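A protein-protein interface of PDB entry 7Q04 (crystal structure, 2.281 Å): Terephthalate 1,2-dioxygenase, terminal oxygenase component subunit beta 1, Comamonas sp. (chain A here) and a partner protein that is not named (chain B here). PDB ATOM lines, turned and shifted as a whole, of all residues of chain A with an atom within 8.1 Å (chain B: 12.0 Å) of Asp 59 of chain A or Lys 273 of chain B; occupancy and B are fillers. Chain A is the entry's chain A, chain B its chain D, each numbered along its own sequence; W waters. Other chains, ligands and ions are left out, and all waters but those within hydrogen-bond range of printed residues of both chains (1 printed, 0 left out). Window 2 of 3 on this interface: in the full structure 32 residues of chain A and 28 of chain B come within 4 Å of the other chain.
The backbone carbonyl oxygen of Cys 34 of chain A sits at hydrogen-bond distance from the backbone NH of Ser 57 of chain A (3.3 Å).
The side-chain hydroxyl of Ser 57 of chain A lies close to the backbone NH of Asp 59 of chain A, 3.4 Å away.
The side-chain carboxylate (OD1) of Asp 274 of chain B lies close to the backbone NH (N) of Ser 276 of chain B (3.0 Å).
OG of Ser 276 of chain B sits at hydrogen-bond distance from NZ of Lys 343 of chain B (2.7 Å).
The backbone carbonyl oxygen (O) of Lys 343 of chain B lies within hydrogen-bond range of the side-chain amide nitrogen (ND2) of Asn 346 of chain B (2.8 Å).
The backbone NH of Phe 353 of chain B is in hydrogen-bond range of the backbone carbonyl oxygen of Asn 346 of chain B (2.9 Å).
Hydrophobic or aromatic side chains of chain A that line the printed part of chain B: Met 60.
Among the printed residues, 12 pairs touch across the chains.
Among the printed residues, Asp or Glu carboxylates within 4 Å of a Lys or Arg side-chain nitrogen of the other chain: Asp 56 of chain A with Lys 343 of chain B.
Phe 30 of chain A touches none of the printed residues of chain B.
No residue of chain B comes within 4 Å of Lys 32 of chain A.
Of the printed residues of chain B, Asp 56 of chain A touches Lys 343 (3.1 Å).
Ser 57 of chain A touches just one residue of chain B: Asp 274.
Asp 59 of chain A touches just these residues of chain B: Lys 273 (3.9 Å) and Asp 274 (3.8 Å).
Met 60 of chain A touches two residues of chain B.
No residue of chain B comes within 4 Å of Leu 61 of chain A.
Thr 62 of chain A touches just one residue of chain B: Lys 273 (3.9 Å).
Asp 63 of chain A touches just these residues of chain B: Leu 272 (3.6 Å), Lys 273 (2.9 Å) and Asp 274 (3.2 Å).
Of the printed residues of chain A, Leu 272 of chain B touches Asp 63 (3.6 Å).
Of chain A, only Asp 59, Thr 62 and Asp 63 come within 4 Å of Lys 273 of chain B.
Printed residues of chain A within 4 Å of Lys 343 of chain B: Asp 56.
Of the printed residues of chain A, Asn 346 of chain B touches Met 60 and Arg 64.
Of the printed residues of chain A, Phe 353 of chain B touches Arg 64 (3.6 Å).
The nearest residue of chain B that does not touch Asp 59 of chain A is Leu 272 of chain B (6.4 Å).
The nearest printed residue of chain B that does not touch Arg 64 of chain A is Lys 343 of chain B (6.8 Å).
Among the printed residues, pairs that only touch across the chains: Met 60 of chain A with Asp 274 of chain B (3.5 Å), Arg 64 of chain A with Phe 353 of chain B (3.6 Å), Asp 63 of chain A with Leu 272 of chain B (3.6 Å), Met 60 of chain A with Asn 346 of chain B (3.8 Å), Asp 59 of chain A with Asp 274 of chain B (3.8 Å), Asp 59 of chain A with Lys 273 of chain B (3.9 Å) and Thr 62 of chain A with Lys 273 of chain B (3.9 Å).
The side-chain amino group (NZ) of Lys 343 of chain B lies within salt-bridge range of the side-chain carboxylate (OD2) of Asp 56 of chain A (3.6 Å).
The side-chain hydroxyl (OG) of Ser 57 of chain A lies within hydrogen-bond range of the side-chain carboxylate (OD2) of Asp 274 of chain B.
OD1 of Asp 63 of chain A lies within hydrogen-bond range of N of Lys 273 of chain B (2.9 Å).
The side-chain carboxylate (OD2) of Asp 63 of chain A is in hydrogen-bond range of the backbone NH (N) of Asp 274 of chain B (3.2 Å).
NH2 of Arg 64 of chain A sits at hydrogen-bond distance from OD1 of Asn 346 of chain B (2.9 Å).
Water W1 lies within hydrogen-bond range of the side-chain carboxylate (OD2) of Asp 274 of chain B (2.5 Å), the side-chain carboxylate (OD1) of Asp 56 of chain A (2.8 Å), the side-chain amino group (NZ) of Lys 343 of chain B (3.0 Å) and the side-chain hydroxyl (OG) of Ser 276 of chain B (3.5 Å).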
ATOM      1  N   PRO A  27      13.745   2.206   2.157  1.00  0.00           N
ATOM      2  CA  PRO A  27      12.569   1.390   1.848  1.00  0.00           C
ATOM      3  C   PRO A  27      11.757   0.911   3.059  1.00  0.00           C
ATOM      4  O   PRO A  27      10.610   0.600   2.882  1.00  0.00           O
ATOM      5  CB  PRO A  27      13.137   0.194   1.088  1.00  0.00           C
ATOM      6  CG  PRO A  27      14.472   0.659   0.568  1.00  0.00           C
ATOM      7  CD  PRO A  27      14.978   1.608   1.635  1.00  0.00           C
ATOM      8  N   PHE A  30       8.173   2.205   3.870  1.00  0.00           N
ATOM      9  CA  PHE A  30       7.073   1.940   2.905  1.00  0.00           C
ATOM     10  C   PHE A  30       6.453   0.561   3.158  1.00  0.00           C
ATOM     11  O   PHE A  30       7.125  -0.338   3.663  1.00  0.00           O
ATOM     12  CB  PHE A  30       7.626   2.046   1.484  1.00  0.00           C
ATOM     13  CG  PHE A  30       8.111   3.420   1.087  1.00  0.00           C
ATOM     14  CD1 PHE A  30       9.392   3.844   1.390  1.00  0.00           C
ATOM     15  CD2 PHE A  30       7.274   4.302   0.428  1.00  0.00           C
ATOM     16  CE1 PHE A  30       9.838   5.105   1.012  1.00  0.00           C
ATOM     17  CE2 PHE A  30       7.731   5.554   0.025  1.00  0.00           C
ATOM     18  CZ  PHE A  30       9.004   5.959   0.339  1.00  0.00           C
ATOM     19  N   THR A  31       5.194   0.383   2.796  1.00  0.00           N
ATOM     20  CA  THR A  31       4.521  -0.933   2.770  1.00  0.00           C
ATOM     21  C   THR A  31       5.090  -1.756   1.616  1.00  0.00           C
ATOM     22  O   THR A  31       5.711  -1.161   0.703  1.00  0.00           O
ATOM     23  CB  THR A  31       3.017  -0.765   2.582  1.00  0.00           C
ATOM     24  OG1 THR A  31       2.805  -0.071   1.342  1.00  0.00           O
ATOM     25  CG2 THR A  31       2.364  -0.051   3.736  1.00  0.00           C
ATOM     26  N   LYS A  32       4.846  -3.066   1.639  1.00  0.00           N
ATOM     27  CA  LYS A  32       5.358  -4.016   0.619  1.00  0.00           C
ATOM     28  C   LYS A  32       4.833  -3.598  -0.772  1.00  0.00           C
ATOM     29  O   LYS A  32       5.613  -3.579  -1.737  1.00  0.00           O
ATOM     30  CB  LYS A  32       4.899  -5.403   1.072  1.00  0.00           C
ATOM     31  CG  LYS A  32       5.956  -6.500   1.092  1.00  0.00           C
ATOM     32  CD  LYS A  32       5.328  -7.908   1.306  1.00  0.00           C
ATOM     33  CE  LYS A  32       5.757  -8.949   0.285  1.00  0.00           C
ATOM     34  NZ  LYS A  32       7.211  -9.245   0.391  1.00  0.00           N
ATOM     35  N   ASP A  33       3.567  -3.191  -0.806  1.00  0.00           N
ATOM     36  CA  ASP A  33       2.724  -2.862  -1.977  1.00  0.00           C
ATOM     37  C   ASP A  33       2.616  -1.335  -2.180  1.00  0.00           C
ATOM     38  O   ASP A  33       1.587  -0.886  -2.625  1.00  0.00           O
ATOM     39  CB  ASP A  33       1.325  -3.486  -1.736  1.00  0.00           C
ATOM     40  CG  ASP A  33       0.527  -2.959  -0.508  1.00  0.00           C
ATOM     41  OD1 ASP A  33       1.147  -2.470   0.469  1.00  0.00           O
ATOM     42  OD2 ASP A  33      -0.734  -3.025  -0.522  1.00  0.00           O
ATOM     43  N   CYS A  34       3.635  -0.556  -1.885  1.00  0.00           N
ATOM     44  CA  CYS A  34       3.591   0.925  -1.843  1.00  0.00           C
ATOM     45  C   CYS A  34       3.751   1.551  -3.232  1.00  0.00           C
ATOM     46  O   CYS A  34       4.198   0.879  -4.155  1.00  0.00           O
ATOM     47  CB  CYS A  34       4.761   1.437  -1.021  1.00  0.00           C
ATOM     48  SG  CYS A  34       6.358   1.130  -1.819  1.00  0.00           S
ATOM     49  N   ALA A  55       7.919   3.739  -8.518  1.00  0.00           N
ATOM     50  CA  ALA A  55       8.019   2.430  -7.847  1.00  0.00           C
ATOM     51  C   ALA A  55       6.647   2.047  -7.342  1.00  0.00           C
ATOM     52  O   ALA A  55       5.960   2.938  -6.832  1.00  0.00           O
ATOM     53  CB  ALA A  55       9.037   2.493  -6.730  1.00  0.00           C
ATOM     54  N   ASP A  56       6.273   0.772  -7.493  1.00  0.00           N
ATOM     55  CA  ASP A  56       4.972   0.216  -7.021  1.00  0.00           C
ATOM     56  C   ASP A  56       5.185  -1.000  -6.110  1.00  0.00           C
ATOM     57  O   ASP A  56       4.223  -1.771  -5.907  1.00  0.00           O
ATOM     58  CB  ASP A  56       4.082  -0.159  -8.204  1.00  0.00           C
ATOM     59  CG  ASP A  56       4.641  -1.264  -9.087  1.00  0.00           C
ATOM     60  OD1 ASP A  56       5.727  -1.781  -8.805  1.00  0.00           O
ATOM     61  OD2 ASP A  56       3.964  -1.602 -10.051  1.00  0.00           O
ATOM     62  N   SER A  57       6.385  -1.149  -5.557  1.00  0.00           N
ATOM     63  CA  SER A  57       6.735  -2.161  -4.537  1.00  0.00           C
ATOM     64  C   SER A  57       7.915  -1.637  -3.712  1.00  0.00           C
ATOM     65  O   SER A  57       8.746  -0.853  -4.250  1.00  0.00           O
ATOM     66  CB  SER A  57       7.078  -3.464  -5.196  1.00  0.00           C
ATOM     67  OG  SER A  57       8.400  -3.428  -5.730  1.00  0.00           O
ATOM     68  N   GLN A  58       8.027  -2.088  -2.469  1.00  0.00           N
ATOM     69  CA  GLN A  58       9.192  -1.754  -1.618  1.00  0.00           C
ATOM     70  C   GLN A  58      10.447  -2.314  -2.285  1.00  0.00           C
ATOM     71  O   GLN A  58      11.519  -1.684  -2.188  1.00  0.00           O
ATOM     72  CB  GLN A  58       8.947  -2.260  -0.204  1.00  0.00           C
ATOM     73  CG  GLN A  58      10.135  -2.055   0.717  1.00  0.00           C
ATOM     74  CD  GLN A  58       9.884  -2.718   2.037  1.00  0.00           C
ATOM     75  OE1 GLN A  58       9.284  -2.148   2.945  1.00  0.00           O
ATOM     76  NE2 GLN A  58      10.346  -3.945   2.135  1.00  0.00           N
ATOM     77  N   ASP A  59      10.317  -3.433  -2.980  1.00  0.00           N
ATOM     78  CA  ASP A  59      11.480  -4.115  -3.613  1.00  0.00           C
ATOM     79  C   ASP A  59      12.098  -3.174  -4.665  1.00  0.00           C
ATOM     80  O   ASP A  59      13.320  -3.154  -4.776  1.00  0.00           O
ATOM     81  CB  ASP A  59      11.107  -5.490  -4.203  1.00  0.00           C
ATOM     82  CG  ASP A  59      10.689  -6.557  -3.204  1.00  0.00           C
ATOM     83  OD1 ASP A  59      10.981  -6.373  -2.018  1.00  0.00           O
ATOM     84  OD2 ASP A  59      10.050  -7.561  -3.635  1.00  0.00           O
ATOM     85  N   MET A  60      11.288  -2.430  -5.424  1.00  0.00           N
ATOM     86  CA  MET A  60      11.809  -1.527  -6.469  1.00  0.00           C
ATOM     87  C   MET A  60      12.633  -0.401  -5.817  1.00  0.00           C
ATOM     88  O   MET A  60      13.573   0.103  -6.455  1.00  0.00           O
ATOM     89  CB  MET A  60      10.671  -0.909  -7.255  1.00  0.00           C
ATOM     90  CG  MET A  60      10.165  -1.802  -8.323  1.00  0.00           C
ATOM     91  SD  MET A  60       9.039  -0.952  -9.465  1.00  0.00           S
ATOM     92  CE  MET A  60      10.249  -0.066 -10.447  1.00  0.00           C
ATOM     93  N   LEU A  61      12.240   0.029  -4.614  1.00  0.00           N
ATOM     94  CA  LEU A  61      12.969   1.051  -3.832  1.00  0.00           C
ATOM     95  C   LEU A  61      14.325   0.447  -3.488  1.00  0.00           C
ATOM     96  O   LEU A  61      15.362   1.128  -3.680  1.00  0.00           O
ATOM     97  CB  LEU A  61      12.173   1.399  -2.569  1.00  0.00           C
ATOM     98  CG  LEU A  61      10.764   1.948  -2.828  1.00  0.00           C
ATOM     99  CD1 LEU A  61      10.084   2.417  -1.541  1.00  0.00           C
ATOM    100  CD2 LEU A  61      10.801   3.070  -3.855  1.00  0.00           C
ATOM    101  N   THR A  62      14.328  -0.801  -3.026  1.00  0.00           N
ATOM    102  CA  THR A  62      15.564  -1.518  -2.606  1.00  0.00           C
ATOM    103  C   THR A  62      16.509  -1.614  -3.809  1.00  0.00           C
ATOM    104  O   THR A  62      17.690  -1.270  -3.633  1.00  0.00           O
ATOM    105  CB  THR A  62      15.238  -2.854  -1.940  1.00  0.00           C
ATOM    106  OG1 THR A  62      14.231  -2.670  -0.952  1.00  0.00           O
ATOM    107  CG2 THR A  62      16.451  -3.444  -1.253  1.00  0.00           C
ATOM    108  N   ASP A  63      15.994  -1.940  -4.993  1.00  0.00           N
ATOM    109  CA  ASP A  63      16.799  -2.034  -6.244  1.00  0.00           C
ATOM    110  C   ASP A  63      17.412  -0.673  -6.613  1.00  0.00           C
ATOM    111  O   ASP A  63      18.585  -0.639  -7.080  1.00  0.00           O
ATOM    112  CB  ASP A  63      15.964  -2.530  -7.427  1.00  0.00           C
ATOM    113  CG  ASP A  63      15.376  -3.904  -7.253  1.00  0.00           C
ATOM    114  OD1 ASP A  63      15.939  -4.675  -6.422  1.00  0.00           O
ATOM    115  OD2 ASP A  63      14.347  -4.158  -7.928  1.00  0.00           O
ATOM    116  N   ARG A  64      16.651   0.408  -6.442  1.00  0.00           N
ATOM    117  CA  ARG A  64      17.127   1.773  -6.787  1.00  0.00           C
ATOM    118  C   ARG A  64      18.362   2.081  -5.935  1.00  0.00           C
ATOM    119  O   ARG A  64      19.341   2.665  -6.462  1.00  0.00           O
ATOM    120  CB  ARG A  64      16.041   2.837  -6.583  1.00  0.00           C
ATOM    121  CG  ARG A  64      16.547   4.254  -6.825  1.00  0.00           C
ATOM    122  CD  ARG A  64      15.464   5.236  -7.174  1.00  0.00           C
ATOM    123  NE  ARG A  64      14.989   5.063  -8.537  1.00  0.00           N
ATOM    124  CZ  ARG A  64      15.596   5.510  -9.623  1.00  0.00           C
ATOM    125  NH1 ARG A  64      16.726   6.181  -9.544  1.00  0.00           N
ATOM    126  NH2 ARG A  64      15.042   5.315 -10.804  1.00  0.00           N
ATOM    127  N   ILE A  65      18.330   1.684  -4.672  1.00  0.00           N
ATOM    128  CA  ILE A  65      19.459   1.941  -3.742  1.00  0.00           C
ATOM    129  C   ILE A  65      20.619   0.992  -4.040  1.00  0.00           C
ATOM    130  O   ILE A  65      21.760   1.484  -4.013  1.00  0.00           O
ATOM    131  CB  ILE A  65      18.994   1.843  -2.294  1.00  0.00           C
ATOM    132  CG1 ILE A  65      18.000   2.967  -2.021  1.00  0.00           C
ATOM    133  CG2 ILE A  65      20.179   1.877  -1.336  1.00  0.00           C
ATOM    134  CD1 ILE A  65      17.089   2.610  -0.900  1.00  0.00           C
ATOM    135  N   SER A  66      20.364  -0.289  -4.336  1.00  0.00           N
ATOM    136  CA  SER A  66      21.437  -1.203  -4.817  1.00  0.00           C
ATOM    137  C   SER A  66      22.175  -0.518  -5.970  1.00  0.00           C
ATOM    138  O   SER A  66      23.402  -0.365  -5.872  1.00  0.00           O
ATOM    139  CB  SER A  66      20.912  -2.549  -5.200  1.00  0.00           C
ATOM    140  OG  SER A  66      20.314  -3.149  -4.059  1.00  0.00           O
ATOM    141  N   TYR B 270      25.064  -8.274  -8.358  1.00  0.00           N
ATOM    142  CA  TYR B 270      23.925  -8.261  -7.398  1.00  0.00           C
ATOM    143  C   TYR B 270      22.609  -8.361  -8.189  1.00  0.00           C
ATOM    144  O   TYR B 270      22.502  -7.727  -9.256  1.00  0.00           O
ATOM    145  CB  TYR B 270      24.005  -7.019  -6.496  1.00  0.00           C
ATOM    146  CG  TYR B 270      25.300  -6.898  -5.725  1.00  0.00           C
ATOM    147  CD1 TYR B 270      26.421  -6.293  -6.286  1.00  0.00           C
ATOM    148  CD2 TYR B 270      25.427  -7.429  -4.446  1.00  0.00           C
ATOM    149  CE1 TYR B 270      27.621  -6.196  -5.591  1.00  0.00           C
ATOM    150  CE2 TYR B 270      26.620  -7.346  -3.739  1.00  0.00           C
ATOM    151  CZ  TYR B 270      27.719  -6.729  -4.314  1.00  0.00           C
ATOM    152  OH  TYR B 270      28.886  -6.661  -3.614  1.00  0.00           O
ATOM    153  N   ARG B 271      21.648  -9.153  -7.695  1.00  0.00           N
ATOM    154  CA  ARG B 271      20.368  -9.470  -8.401  1.00  0.00           C
ATOM    155  C   ARG B 271      19.290  -8.470  -7.947  1.00  0.00           C
ATOM    156  O   ARG B 271      19.355  -7.961  -6.800  1.00  0.00           O
ATOM    157  CB  ARG B 271      19.927 -10.931  -8.182  1.00  0.00           C
ATOM    158  CG  ARG B 271      19.547 -11.720  -9.437  1.00  0.00           C
ATOM    159  CD  ARG B 271      20.608 -11.758 -10.545  1.00  0.00           C
ATOM    160  NE  ARG B 271      22.012 -11.860 -10.103  1.00  0.00           N
ATOM    161  CZ  ARG B 271      22.688 -12.984  -9.820  1.00  0.00           C
ATOM    162  NH1 ARG B 271      22.100 -14.165  -9.897  1.00  0.00           N
ATOM    163  NH2 ARG B 271      23.954 -12.918  -9.435  1.00  0.00           N
ATOM    164  N   LEU B 272      18.329  -8.191  -8.839  1.00  0.00           N
ATOM    165  CA  LEU B 272      17.150  -7.311  -8.602  1.00  0.00           C
ATOM    166  C   LEU B 272      16.114  -8.084  -7.794  1.00  0.00           C
ATOM    167  O   LEU B 272      15.709  -9.151  -8.291  1.00  0.00           O
ATOM    168  CB  LEU B 272      16.529  -6.908  -9.942  1.00  0.00           C
ATOM    169  CG  LEU B 272      17.074  -5.635 -10.587  1.00  0.00           C
ATOM    170  CD1 LEU B 272      18.603  -5.560 -10.502  1.00  0.00           C
ATOM    171  CD2 LEU B 272      16.604  -5.543 -12.033  1.00  0.00           C
ATOM    172  N   LYS B 273      15.641  -7.536  -6.669  1.00  0.00           N
ATOM    173  CA  LYS B 273      14.542  -8.131  -5.868  1.00  0.00           C
ATOM    174  C   LYS B 273      13.233  -8.029  -6.656  1.00  0.00           C
ATOM    175  O   LYS B 273      12.347  -8.877  -6.444  1.00  0.00           O
ATOM    176  CB  LYS B 273      14.421  -7.461  -4.498  1.00  0.00           C
ATOM    177  CG  LYS B 273      15.671  -7.519  -3.638  1.00  0.00           C
ATOM    178  CD  LYS B 273      15.393  -7.254  -2.165  1.00  0.00           C
ATOM    179  CE  LYS B 273      16.643  -7.314  -1.304  1.00  0.00           C
ATOM    180  NZ  LYS B 273      17.316  -8.633  -1.405  1.00  0.00           N
ATOM    181  N   ASP B 274      13.115  -7.044  -7.545  1.00  0.00           N
ATOM    182  CA  ASP B 274      11.919  -6.873  -8.403  1.00  0.00           C
ATOM    183  C   ASP B 274      12.363  -6.786  -9.856  1.00  0.00           C
ATOM    184  O   ASP B 274      12.534  -5.691 -10.387  1.00  0.00           O
ATOM    185  CB  ASP B 274      11.105  -5.652  -7.976  1.00  0.00           C
ATOM    186  CG  ASP B 274       9.774  -5.542  -8.699  1.00  0.00           C
ATOM    187  OD1 ASP B 274       9.695  -6.037  -9.844  1.00  0.00           O
ATOM    188  OD2 ASP B 274       8.833  -4.980  -8.101  1.00  0.00           O
ATOM    189  N   PRO B 275      12.533  -7.932 -10.552  1.00  0.00           N
ATOM    190  CA  PRO B 275      13.017  -7.910 -11.937  1.00  0.00           C
ATOM    191  C   PRO B 275      12.021  -7.283 -12.934  1.00  0.00           C
ATOM    192  O   PRO B 275      12.420  -7.057 -14.070  1.00  0.00           O
ATOM    193  CB  PRO B 275      13.286  -9.384 -12.265  1.00  0.00           C
ATOM    194  CG  PRO B 275      13.217 -10.118 -10.918  1.00  0.00           C
ATOM    195  CD  PRO B 275      12.288  -9.293 -10.046  1.00  0.00           C
ATOM    196  N   SER B 276      10.779  -7.006 -12.490  1.00  0.00           N
ATOM    197  CA  SER B 276       9.681  -6.388 -13.289  1.00  0.00           C
ATOM    198  C   SER B 276      10.148  -5.093 -13.981  1.00  0.00           C
ATOM    199  O   SER B 276       9.547  -4.725 -15.005  1.00  0.00           O
ATOM    200  CB  SER B 276       8.425  -6.153 -12.451  1.00  0.00           C
ATOM    201  OG  SER B 276       8.513  -4.996 -11.630  1.00  0.00           O
ATOM    202  N   LEU B 277      11.164  -4.407 -13.439  1.00  0.00           N
ATOM    203  CA  LEU B 277      11.766  -3.191 -14.053  1.00  0.00           C
ATOM    204  C   LEU B 277      12.169  -3.476 -15.510  1.00  0.00           C
ATOM    205  O   LEU B 277      12.013  -2.562 -16.339  1.00  0.00           O
ATOM    206  CB  LEU B 277      12.961  -2.742 -13.214  1.00  0.00           C
ATOM    207  CG  LEU B 277      13.969  -1.839 -13.922  1.00  0.00           C
ATOM    208  CD1 LEU B 277      13.394  -0.458 -14.192  1.00  0.00           C
ATOM    209  CD2 LEU B 277      15.238  -1.723 -13.086  1.00  0.00           C
ATOM    210  N   LEU B 278      12.654  -4.681 -15.821  1.00  0.00           N
ATOM    211  CA  LEU B 278      13.146  -5.032 -17.183  1.00  0.00           C
ATOM    212  C   LEU B 278      12.164  -5.963 -17.903  1.00  0.00           C
ATOM    213  O   LEU B 278      12.429  -6.257 -19.087  1.00  0.00           O
ATOM    214  CB  LEU B 278      14.522  -5.694 -17.071  1.00  0.00           C
ATOM    215  CG  LEU B 278      15.587  -4.853 -16.392  1.00  0.00           C
ATOM    216  CD1 LEU B 278      16.881  -5.641 -16.271  1.00  0.00           C
ATOM    217  CD2 LEU B 278      15.793  -3.556 -17.151  1.00  0.00           C
ATOM    218  N   GLU B 279      11.109  -6.431 -17.225  1.00  0.00           N
ATOM    219  CA  GLU B 279      10.041  -7.272 -17.838  1.00  0.00           C
ATOM    220  C   GLU B 279       9.336  -6.415 -18.892  1.00  0.00           C
ATOM    221  O   GLU B 279       8.566  -5.496 -18.510  1.00  0.00           O
ATOM    222  CB  GLU B 279       9.064  -7.847 -16.809  1.00  0.00           C
ATOM    223  CG  GLU B 279       9.334  -9.311 -16.487  1.00  0.00           C
ATOM    224  CD  GLU B 279       8.988  -9.738 -15.070  1.00  0.00           C
ATOM    225  OE1 GLU B 279       8.005  -9.193 -14.488  1.00  0.00           O
ATOM    226  OE2 GLU B 279       9.706 -10.622 -14.551  1.00  0.00           O
ATOM    227  N   LYS B 343       7.423   1.831 -15.372  1.00  0.00           N
ATOM    228  CA  LYS B 343       8.521   1.153 -14.634  1.00  0.00           C
ATOM    229  C   LYS B 343       9.835   1.343 -15.384  1.00  0.00           C
ATOM    230  O   LYS B 343      10.815   1.677 -14.764  1.00  0.00           O
ATOM    231  CB  LYS B 343       8.274  -0.340 -14.462  1.00  0.00           C
ATOM    232  CG  LYS B 343       7.127  -0.701 -13.530  1.00  0.00           C
ATOM    233  CD  LYS B 343       7.203  -2.122 -12.978  1.00  0.00           C
ATOM    234  CE  LYS B 343       5.905  -2.574 -12.332  1.00  0.00           C
ATOM    235  NZ  LYS B 343       6.005  -3.949 -11.768  1.00  0.00           N
ATOM    236  N   ASN B 346      12.343   4.496 -15.232  1.00  0.00           N
ATOM    237  CA  ASN B 346      13.411   4.554 -14.211  1.00  0.00           C
ATOM    238  C   ASN B 346      14.777   4.421 -14.882  1.00  0.00           C
ATOM    239  O   ASN B 346      15.772   4.714 -14.212  1.00  0.00           O
ATOM    240  CB  ASN B 346      13.248   3.474 -13.149  1.00  0.00           C
ATOM    241  CG  ASN B 346      12.109   3.778 -12.208  1.00  0.00           C
ATOM    242  OD1 ASN B 346      12.262   4.616 -11.333  1.00  0.00           O
ATOM    243  ND2 ASN B 346      10.985   3.101 -12.353  1.00  0.00           N
ATOM    244  N   PHE B 353      18.704   4.807 -14.365  1.00  0.00           N
ATOM    245  CA  PHE B 353      19.741   3.765 -14.156  1.00  0.00           C
ATOM    246  C   PHE B 353      20.757   3.855 -15.307  1.00  0.00           C
ATOM    247  O   PHE B 353      21.963   3.791 -15.039  1.00  0.00           O
ATOM    248  CB  PHE B 353      19.102   2.391 -14.012  1.00  0.00           C
ATOM    249  CG  PHE B 353      18.165   2.275 -12.833  1.00  0.00           C
ATOM    250  CD1 PHE B 353      18.512   2.779 -11.589  1.00  0.00           C
ATOM    251  CD2 PHE B 353      16.940   1.625 -12.947  1.00  0.00           C
ATOM    252  CE1 PHE B 353      17.658   2.642 -10.501  1.00  0.00           C
ATOM    253  CE2 PHE B 353      16.081   1.510 -11.864  1.00  0.00           C
ATOM    254  CZ  PHE B 353      16.439   2.023 -10.645  1.00  0.00           C
HETATM  255  O   HOH W   1       6.528  -4.448  -8.834  1.00  0.00           O
